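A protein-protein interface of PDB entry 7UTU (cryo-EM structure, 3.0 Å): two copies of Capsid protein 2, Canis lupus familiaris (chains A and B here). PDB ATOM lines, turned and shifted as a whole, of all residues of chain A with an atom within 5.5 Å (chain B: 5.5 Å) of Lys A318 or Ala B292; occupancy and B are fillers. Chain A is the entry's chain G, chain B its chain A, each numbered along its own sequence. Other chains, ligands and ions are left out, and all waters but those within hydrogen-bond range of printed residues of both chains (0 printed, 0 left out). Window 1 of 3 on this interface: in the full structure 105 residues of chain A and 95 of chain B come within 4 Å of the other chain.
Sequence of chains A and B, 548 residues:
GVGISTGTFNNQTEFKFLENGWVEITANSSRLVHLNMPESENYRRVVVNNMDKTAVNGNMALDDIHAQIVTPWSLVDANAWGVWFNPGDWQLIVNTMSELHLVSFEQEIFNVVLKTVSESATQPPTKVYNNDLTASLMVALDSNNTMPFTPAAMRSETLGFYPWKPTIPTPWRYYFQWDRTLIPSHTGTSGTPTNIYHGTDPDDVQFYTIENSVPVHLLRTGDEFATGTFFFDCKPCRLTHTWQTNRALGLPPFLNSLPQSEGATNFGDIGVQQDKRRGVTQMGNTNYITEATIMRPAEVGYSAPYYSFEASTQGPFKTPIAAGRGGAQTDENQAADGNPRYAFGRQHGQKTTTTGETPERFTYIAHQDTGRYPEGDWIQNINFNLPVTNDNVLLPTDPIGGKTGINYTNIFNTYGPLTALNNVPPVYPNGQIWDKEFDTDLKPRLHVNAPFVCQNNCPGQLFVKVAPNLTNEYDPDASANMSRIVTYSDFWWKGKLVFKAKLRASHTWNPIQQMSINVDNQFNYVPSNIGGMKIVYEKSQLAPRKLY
Of the printed residues of chain B, Lys A318 touches Gln B282 (3.5 Å) and Ala B292 (3.2 Å). Printed residues of chain A within 4 Å of Ala B292: Ala A61, Asp A63, Phe A309, Pro A316 and Lys A318. Printed residues of chain A within 4 Å of Arg B247: Asp A63 and Pro A316. Printed residues of chain A within 4 Å of Glu B291: Asp A63. Of the printed residues of chain A, Met B283 touches Tyr A307 (3.5 Å) and Phe A309 (3.9 Å). Printed residues of chain B within 4 Å of Ala A61: Thr B290 (3.2 Å) and Ala B292 (3.5 Å). The nearest printed residue of chain B that does not touch Lys A318 is Met B283 (4.01 Å). The nearest printed residue of chain A that does not touch Ala B292 is Phe A317 (4.001 Å). The nearest printed residue of chain A that does not touch Arg B247 is Phe A317 (4.1 Å).
No position is printed for both chains. Of the 17 pairs that touch across the chains among the printed residues, none has its exchanged pair printed and touching as well.
The backbone carbonyl oxygen of Asn B246 sits at hydrogen-bond distance from the guanidinium group of Arg B296, 3.1 Å away. O of Arg B247 lies within hydrogen-bond range of NH2 of Arg B296 (2.6 Å). The side-chain carboxylate (OE1) of Glu B291 lies within salt-bridge range of the guanidinium group (NH2) of Arg B296 (3.5 Å). The backbone NH (N) of Glu A310 sits at hydrogen-bond distance from the backbone carbonyl oxygen (O) of Phe A317 (3.0 Å).
Among the printed residues, merely in contact across the chains: Ala A61 with Thr B290 (3.2 Å), Phe A317 with Asn B246 (3.2 Å), Phe A309 with Ala B292 (3.3 Å), Pro A320 with Gln B282 (3.3 Å), Asp A63 with Glu B291 (3.5 Å), Ala A61 with Ala B292 (3.5 Å), Lys A318 with Gln B282 (3.5 Å), Tyr A307 with Met B283 (3.5 Å), Asp A63 with Thr B290 (3.5 Å), Pro A316 with Ala B292 (3.7 Å), Asp A63 with Ala B292 (3.8 Å), Leu A62 with Thr B290 (3.8 Å) and Phe A309 with Met B283 (3.9 Å).
OD1 of Asp A63 lies within salt-bridge range of NH2 of Arg B247 (2.8 Å). The backbone carbonyl oxygen (O) of Ile A321 lies within hydrogen-bond range of the side-chain amide nitrogen (NE2) of Gln B282, at 2.9 Å. N of Lys A318 is in hydrogen-bond range of O of Ala B292 (3.2 Å). The backbone carbonyl oxygen (O) of Pro A316 sits close to the guanidinium group (NH1) of Arg B247 (2.4 Å).
Of the 10 printed residues of chain B, 7 touch a printed residue of chain A. Printed residues of chain B that touch a printed residue of chain A: Asn B246, Arg B247, Gln B282, Met B283, Thr B290, Glu B291 and Ala B292. Hydrophobic or aromatic side chains of chain B that line the printed part of chain A: Met B283 and Ala B292. Among the printed residues, 17 pairs touch across the chains.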
ATOM      1  N   MET A  60      -5.546 -13.069  21.125  1.00  0.00           N
ATOM      2  CA  MET A  60      -6.082 -14.370  21.521  1.00  0.00           C
ATOM      3  C   MET A  60      -5.250 -14.986  22.636  1.00  0.00           C
ATOM      4  O   MET A  60      -5.790 -15.617  23.551  1.00  0.00           O
ATOM      5  CB  MET A  60      -6.127 -15.336  20.330  1.00  0.00           C
ATOM      6  CG  MET A  60      -6.596 -14.807  18.961  1.00  0.00           C
ATOM      7  SD  MET A  60      -5.530 -15.326  17.598  1.00  0.00           S
ATOM      8  CE  MET A  60      -3.970 -14.526  17.988  1.00  0.00           C
ATOM      9  N   ALA A  61      -3.928 -14.813  22.575  1.00  0.00           N
ATOM     10  CA  ALA A  61      -3.033 -15.436  23.542  1.00  0.00           C
ATOM     11  C   ALA A  61      -3.162 -14.855  24.945  1.00  0.00           C
ATOM     12  O   ALA A  61      -2.662 -15.467  25.895  1.00  0.00           O
ATOM     13  CB  ALA A  61      -1.587 -15.304  23.065  1.00  0.00           C
ATOM     14  N   LEU A  62      -3.818 -13.705  25.107  1.00  0.00           N
ATOM     15  CA  LEU A  62      -3.942 -13.033  26.394  1.00  0.00           C
ATOM     16  C   LEU A  62      -5.185 -13.459  27.169  1.00  0.00           C
ATOM     17  O   LEU A  62      -5.711 -12.668  27.959  1.00  0.00           O
ATOM     18  CB  LEU A  62      -3.960 -11.517  26.183  1.00  0.00           C
ATOM     19  CG  LEU A  62      -2.821 -10.917  25.354  1.00  0.00           C
ATOM     20  CD1 LEU A  62      -3.002  -9.417  25.198  1.00  0.00           C
ATOM     21  CD2 LEU A  62      -1.463 -11.226  25.967  1.00  0.00           C
ATOM     22  N   ASP A  63      -5.660 -14.681  26.959  1.00  0.00           N
ATOM     23  CA  ASP A  63      -6.868 -15.191  27.597  1.00  0.00           C
ATOM     24  C   ASP A  63      -6.518 -15.650  29.006  1.00  0.00           C
ATOM     25  O   ASP A  63      -5.899 -16.701  29.187  1.00  0.00           O
ATOM     26  CB  ASP A  63      -7.432 -16.328  26.749  1.00  0.00           C
ATOM     27  CG  ASP A  63      -8.818 -16.783  27.181  1.00  0.00           C
ATOM     28  OD1 ASP A  63      -9.083 -16.939  28.392  1.00  0.00           O
ATOM     29  OD2 ASP A  63      -9.665 -16.991  26.287  1.00  0.00           O
ATOM     30  N   PRO A 305       5.056 -28.680  16.429  1.00  0.00           N
ATOM     31  CA  PRO A 305       4.566 -27.378  15.961  1.00  0.00           C
ATOM     32  C   PRO A 305       4.780 -26.276  16.983  1.00  0.00           C
ATOM     33  O   PRO A 305       4.171 -26.306  18.058  1.00  0.00           O
ATOM     34  CB  PRO A 305       3.077 -27.638  15.712  1.00  0.00           C
ATOM     35  CG  PRO A 305       2.745 -28.747  16.603  1.00  0.00           C
ATOM     36  CD  PRO A 305       3.941 -29.619  16.640  1.00  0.00           C
ATOM     37  N   TYR A 306       5.624 -25.298  16.657  1.00  0.00           N
ATOM     38  CA  TYR A 306       6.052 -24.315  17.645  1.00  0.00           C
ATOM     39  C   TYR A 306       5.103 -23.124  17.663  1.00  0.00           C
ATOM     40  O   TYR A 306       4.617 -22.676  16.620  1.00  0.00           O
ATOM     41  CB  TYR A 306       7.508 -23.872  17.413  1.00  0.00           C
ATOM     42  CG  TYR A 306       7.957 -23.515  16.006  1.00  0.00           C
ATOM     43  CD1 TYR A 306       9.080 -24.114  15.463  1.00  0.00           C
ATOM     44  CD2 TYR A 306       7.334 -22.522  15.265  1.00  0.00           C
ATOM     45  CE1 TYR A 306       9.516 -23.799  14.200  1.00  0.00           C
ATOM     46  CE2 TYR A 306       7.774 -22.190  14.002  1.00  0.00           C
ATOM     47  CZ  TYR A 306       8.867 -22.830  13.475  1.00  0.00           C
ATOM     48  OH  TYR A 306       9.305 -22.498  12.215  1.00  0.00           O
ATOM     49  N   TYR A 307       4.821 -22.640  18.875  1.00  0.00           N
ATOM     50  CA  TYR A 307       3.842 -21.576  19.123  1.00  0.00           C
ATOM     51  C   TYR A 307       2.493 -21.939  18.505  1.00  0.00           C
ATOM     52  O   TYR A 307       1.840 -21.130  17.843  1.00  0.00           O
ATOM     53  CB  TYR A 307       4.355 -20.214  18.629  1.00  0.00           C
ATOM     54  CG  TYR A 307       5.400 -19.536  19.514  1.00  0.00           C
ATOM     55  CD1 TYR A 307       6.195 -20.253  20.403  1.00  0.00           C
ATOM     56  CD2 TYR A 307       5.581 -18.161  19.456  1.00  0.00           C
ATOM     57  CE1 TYR A 307       7.131 -19.629  21.192  1.00  0.00           C
ATOM     58  CE2 TYR A 307       6.520 -17.529  20.246  1.00  0.00           C
ATOM     59  CZ  TYR A 307       7.293 -18.268  21.106  1.00  0.00           C
ATOM     60  OH  TYR A 307       8.226 -17.644  21.902  1.00  0.00           O
ATOM     61  N   SER A 308       2.091 -23.189  18.723  1.00  0.00           N
ATOM     62  CA  SER A 308       0.769 -23.668  18.351  1.00  0.00           C
ATOM     63  C   SER A 308      -0.123 -23.650  19.580  1.00  0.00           C
ATOM     64  O   SER A 308       0.282 -24.107  20.652  1.00  0.00           O
ATOM     65  CB  SER A 308       0.854 -25.082  17.782  1.00  0.00           C
ATOM     66  OG  SER A 308      -0.311 -25.826  18.087  1.00  0.00           O
ATOM     67  N   PHE A 309      -1.331 -23.118  19.420  1.00  0.00           N
ATOM     68  CA  PHE A 309      -2.316 -23.019  20.485  1.00  0.00           C
ATOM     69  C   PHE A 309      -3.506 -23.888  20.120  1.00  0.00           C
ATOM     70  O   PHE A 309      -4.030 -23.785  19.007  1.00  0.00           O
ATOM     71  CB  PHE A 309      -2.753 -21.571  20.689  1.00  0.00           C
ATOM     72  CG  PHE A 309      -1.701 -20.709  21.318  1.00  0.00           C
ATOM     73  CD1 PHE A 309      -0.710 -20.137  20.547  1.00  0.00           C
ATOM     74  CD2 PHE A 309      -1.700 -20.476  22.677  1.00  0.00           C
ATOM     75  CE1 PHE A 309       0.261 -19.350  21.120  1.00  0.00           C
ATOM     76  CE2 PHE A 309      -0.732 -19.688  23.253  1.00  0.00           C
ATOM     77  CZ  PHE A 309       0.250 -19.125  22.473  1.00  0.00           C
ATOM     78  N   GLU A 310      -3.918 -24.744  21.058  1.00  0.00           N
ATOM     79  CA  GLU A 310      -5.026 -25.670  20.878  1.00  0.00           C
ATOM     80  C   GLU A 310      -6.113 -25.402  21.906  1.00  0.00           C
ATOM     81  O   GLU A 310      -5.830 -25.105  23.069  1.00  0.00           O
ATOM     82  CB  GLU A 310      -4.600 -27.138  20.977  1.00  0.00           C
ATOM     83  CG  GLU A 310      -3.313 -27.501  20.260  1.00  0.00           C
ATOM     84  CD  GLU A 310      -2.895 -28.938  20.500  1.00  0.00           C
ATOM     85  OE1 GLU A 310      -3.303 -29.524  21.523  1.00  0.00           O
ATOM     86  OE2 GLU A 310      -2.158 -29.486  19.659  1.00  0.00           O
ATOM     87  N   PRO A 316      -8.193 -21.810  25.018  1.00  0.00           N
ATOM     88  CA  PRO A 316      -6.929 -22.165  24.368  1.00  0.00           C
ATOM     89  C   PRO A 316      -5.735 -22.168  25.306  1.00  0.00           C
ATOM     90  O   PRO A 316      -5.709 -21.485  26.332  1.00  0.00           O
ATOM     91  CB  PRO A 316      -6.781 -21.084  23.294  1.00  0.00           C
ATOM     92  CG  PRO A 316      -7.464 -19.917  23.850  1.00  0.00           C
ATOM     93  CD  PRO A 316      -8.618 -20.444  24.659  1.00  0.00           C
ATOM     94  N   PHE A 317      -4.733 -22.962  24.929  1.00  0.00           N
ATOM     95  CA  PHE A 317      -3.502 -23.089  25.693  1.00  0.00           C
ATOM     96  C   PHE A 317      -2.367 -23.472  24.757  1.00  0.00           C
ATOM     97  O   PHE A 317      -2.596 -24.009  23.670  1.00  0.00           O
ATOM     98  CB  PHE A 317      -3.634 -24.122  26.817  1.00  0.00           C
ATOM     99  CG  PHE A 317      -3.926 -25.516  26.337  1.00  0.00           C
ATOM    100  CD1 PHE A 317      -5.223 -25.917  26.089  1.00  0.00           C
ATOM    101  CD2 PHE A 317      -2.905 -26.431  26.156  1.00  0.00           C
ATOM    102  CE1 PHE A 317      -5.495 -27.196  25.653  1.00  0.00           C
ATOM    103  CE2 PHE A 317      -3.172 -27.708  25.719  1.00  0.00           C
ATOM    104  CZ  PHE A 317      -4.467 -28.092  25.471  1.00  0.00           C
ATOM    105  N   LYS A 318      -1.141 -23.210  25.200  1.00  0.00           N
ATOM    106  CA  LYS A 318       0.037 -23.475  24.385  1.00  0.00           C
ATOM    107  C   LYS A 318       0.459 -24.934  24.506  1.00  0.00           C
ATOM    108  O   LYS A 318       0.423 -25.512  25.595  1.00  0.00           O
ATOM    109  CB  LYS A 318       1.177 -22.550  24.811  1.00  0.00           C
ATOM    110  CG  LYS A 318       2.443 -22.674  23.979  1.00  0.00           C
ATOM    111  CD  LYS A 318       3.539 -23.422  24.734  1.00  0.00           C
ATOM    112  CE  LYS A 318       4.851 -23.508  23.955  1.00  0.00           C
ATOM    113  NZ  LYS A 318       4.694 -23.855  22.515  1.00  0.00           N
ATOM    114  N   THR A 319       0.863 -25.522  23.387  1.00  0.00           N
ATOM    115  CA  THR A 319       1.332 -26.905  23.379  1.00  0.00           C
ATOM    116  C   THR A 319       2.739 -26.965  23.961  1.00  0.00           C
ATOM    117  O   THR A 319       3.642 -26.333  23.398  1.00  0.00           O
ATOM    118  CB  THR A 319       1.359 -27.462  21.963  1.00  0.00           C
ATOM    119  OG1 THR A 319       2.197 -26.641  21.140  1.00  0.00           O
ATOM    120  CG2 THR A 319      -0.019 -27.504  21.380  1.00  0.00           C
ATOM    121  N   PRO A 320       2.998 -27.698  25.044  1.00  0.00           N
ATOM    122  CA  PRO A 320       4.373 -27.763  25.535  1.00  0.00           C
ATOM    123  C   PRO A 320       5.250 -28.613  24.629  1.00  0.00           C
ATOM    124  O   PRO A 320       4.798 -29.566  23.991  1.00  0.00           O
ATOM    125  CB  PRO A 320       4.230 -28.384  26.926  1.00  0.00           C
ATOM    126  CG  PRO A 320       3.024 -29.193  26.839  1.00  0.00           C
ATOM    127  CD  PRO A 320       2.095 -28.440  25.945  1.00  0.00           C
ATOM    128  N   ILE A 321       6.530 -28.244  24.590  1.00  0.00           N
ATOM    129  CA  ILE A 321       7.552 -28.912  23.792  1.00  0.00           C
ATOM    130  C   ILE A 321       8.631 -29.406  24.742  1.00  0.00           C
ATOM    131  O   ILE A 321       9.080 -28.666  25.624  1.00  0.00           O
ATOM    132  CB  ILE A 321       8.169 -27.984  22.717  1.00  0.00           C
ATOM    133  CG1 ILE A 321       7.107 -27.141  21.982  1.00  0.00           C
ATOM    134  CG2 ILE A 321       8.984 -28.800  21.709  1.00  0.00           C
ATOM    135  CD1 ILE A 321       6.047 -27.931  21.218  1.00  0.00           C
ATOM    136  N   ASN B 246      -5.669 -28.754  30.279  1.00  0.00           N
ATOM    137  CA  ASN B 246      -4.408 -28.086  30.608  1.00  0.00           C
ATOM    138  C   ASN B 246      -4.620 -26.782  31.361  1.00  0.00           C
ATOM    139  O   ASN B 246      -3.831 -26.434  32.247  1.00  0.00           O
ATOM    140  CB  ASN B 246      -3.613 -27.795  29.337  1.00  0.00           C
ATOM    141  CG  ASN B 246      -2.727 -28.938  28.927  1.00  0.00           C
ATOM    142  OD1 ASN B 246      -3.063 -30.107  29.117  1.00  0.00           O
ATOM    143  ND2 ASN B 246      -1.569 -28.605  28.371  1.00  0.00           N
ATOM    144  N   ARG B 247      -5.672 -26.043  31.017  1.00  0.00           N
ATOM    145  CA  ARG B 247      -5.907 -24.760  31.663  1.00  0.00           C
ATOM    146  C   ARG B 247      -6.239 -24.910  33.140  1.00  0.00           C
ATOM    147  O   ARG B 247      -5.953 -24.004  33.930  1.00  0.00           O
ATOM    148  CB  ARG B 247      -7.025 -24.016  30.934  1.00  0.00           C
ATOM    149  CG  ARG B 247      -6.623 -23.370  29.616  1.00  0.00           C
ATOM    150  CD  ARG B 247      -5.716 -22.146  29.811  1.00  0.00           C
ATOM    151  NE  ARG B 247      -6.445 -20.893  29.975  1.00  0.00           N
ATOM    152  CZ  ARG B 247      -7.242 -20.331  29.077  1.00  0.00           C
ATOM    153  NH1 ARG B 247      -7.386 -20.829  27.861  1.00  0.00           N
ATOM    154  NH2 ARG B 247      -7.889 -19.216  29.397  1.00  0.00           N
ATOM    155  N   GLN B 282       7.204 -21.359  28.881  1.00  0.00           N
ATOM    156  CA  GLN B 282       8.089 -21.941  27.881  1.00  0.00           C
ATOM    157  C   GLN B 282       8.423 -20.977  26.749  1.00  0.00           C
ATOM    158  O   GLN B 282       9.486 -21.107  26.146  1.00  0.00           O
ATOM    159  CB  GLN B 282       7.478 -23.195  27.252  1.00  0.00           C
ATOM    160  CG  GLN B 282       8.090 -24.489  27.716  1.00  0.00           C
ATOM    161  CD  GLN B 282       7.494 -25.688  27.019  1.00  0.00           C
ATOM    162  OE1 GLN B 282       6.822 -25.541  26.001  1.00  0.00           O
ATOM    163  NE2 GLN B 282       7.746 -26.883  27.543  1.00  0.00           N
ATOM    164  N   MET B 283       7.549 -20.012  26.456  1.00  0.00           N
ATOM    165  CA  MET B 283       7.723 -19.169  25.283  1.00  0.00           C
ATOM    166  C   MET B 283       8.739 -18.082  25.651  1.00  0.00           C
ATOM    167  O   MET B 283       8.416 -16.963  26.058  1.00  0.00           O
ATOM    168  CB  MET B 283       6.393 -18.634  24.754  1.00  0.00           C
ATOM    169  CG  MET B 283       5.141 -19.558  24.950  1.00  0.00           C
ATOM    170  SD  MET B 283       3.509 -18.864  24.637  1.00  0.00           S
ATOM    171  CE  MET B 283       3.829 -17.691  23.338  1.00  0.00           C
ATOM    172  N   THR B 290       0.565 -15.392  31.026  1.00  0.00           N
ATOM    173  CA  THR B 290      -0.885 -15.489  31.012  1.00  0.00           C
ATOM    174  C   THR B 290      -1.251 -16.960  30.923  1.00  0.00           C
ATOM    175  O   THR B 290      -0.390 -17.821  30.733  1.00  0.00           O
ATOM    176  CB  THR B 290      -1.513 -14.688  29.863  1.00  0.00           C
ATOM    177  OG1 THR B 290      -2.929 -14.895  29.860  1.00  0.00           O
ATOM    178  CG2 THR B 290      -0.939 -15.063  28.501  1.00  0.00           C
ATOM    179  N   GLU B 291      -2.546 -17.238  31.058  1.00  0.00           N
ATOM    180  CA  GLU B 291      -2.986 -18.614  31.234  1.00  0.00           C
ATOM    181  C   GLU B 291      -2.805 -19.455  29.981  1.00  0.00           C
ATOM    182  O   GLU B 291      -2.631 -20.673  30.093  1.00  0.00           O
ATOM    183  CB  GLU B 291      -4.457 -18.636  31.658  1.00  0.00           C
ATOM    184  CG  GLU B 291      -4.859 -18.330  33.122  1.00  0.00           C
ATOM    185  CD  GLU B 291      -4.080 -19.016  34.251  1.00  0.00           C
ATOM    186  OE1 GLU B 291      -3.025 -19.651  34.083  1.00  0.00           O
ATOM    187  OE2 GLU B 291      -4.583 -18.923  35.381  1.00  0.00           O
ATOM    188  N   ALA B 292      -2.846 -18.847  28.795  1.00  0.00           N
ATOM    189  CA  ALA B 292      -2.473 -19.567  27.583  1.00  0.00           C
ATOM    190  C   ALA B 292      -0.961 -19.703  27.420  1.00  0.00           C
ATOM    191  O   ALA B 292      -0.519 -20.372  26.483  1.00  0.00           O
ATOM    192  CB  ALA B 292      -3.066 -18.874  26.356  1.00  0.00           C
ATOM    193  N   THR B 293      -0.168 -19.093  28.311  1.00  0.00           N
ATOM    194  CA  THR B 293       1.283 -19.065  28.239  1.00  0.00           C
ATOM    195  C   THR B 293       1.986 -19.782  29.378  1.00  0.00           C
ATOM    196  O   THR B 293       3.104 -20.262  29.173  1.00  0.00           O
ATOM    197  CB  THR B 293       1.775 -17.609  28.208  1.00  0.00           C
ATOM    198  OG1 THR B 293       1.050 -16.874  27.214  1.00  0.00           O
ATOM    199  CG2 THR B 293       3.267 -17.520  27.978  1.00  0.00           C
ATOM    200  N   ILE B 294       1.376 -19.877  30.558  1.00  0.00           N
ATOM    201  CA  ILE B 294       2.087 -20.403  31.717  1.00  0.00           C
ATOM    202  C   ILE B 294       2.293 -21.903  31.554  1.00  0.00           C
ATOM    203  O   ILE B 294       1.405 -22.623  31.079  1.00  0.00           O
ATOM    204  CB  ILE B 294       1.335 -20.058  33.015  1.00  0.00           C
ATOM    205  CG1 ILE B 294       2.216 -20.340  34.235  1.00  0.00           C
ATOM    206  CG2 ILE B 294       0.015 -20.819  33.126  1.00  0.00           C
ATOM    207  CD1 ILE B 294       1.648 -19.821  35.541  1.00  0.00           C
ATOM    208  N   ARG B 296       2.537 -25.794  32.102  1.00  0.00           N
ATOM    209  CA  ARG B 296       1.833 -26.864  32.787  1.00  0.00           C
ATOM    210  C   ARG B 296       2.644 -28.148  32.655  1.00  0.00           C
ATOM    211  O   ARG B 296       3.497 -28.251  31.765  1.00  0.00           O
ATOM    212  CB  ARG B 296       0.421 -27.066  32.214  1.00  0.00           C
ATOM    213  CG  ARG B 296      -0.414 -25.796  32.075  1.00  0.00           C
ATOM    214  CD  ARG B 296      -0.521 -25.022  33.385  1.00  0.00           C
ATOM    215  NE  ARG B 296      -1.844 -24.465  33.642  1.00  0.00           N
ATOM    216  CZ  ARG B 296      -2.425 -23.498  32.944  1.00  0.00           C
ATOM    217  NH1 ARG B 296      -1.884 -23.007  31.839  1.00  0.00           N
ATOM    218  NH2 ARG B 296      -3.582 -23.002  33.371  1.00  0.00           N
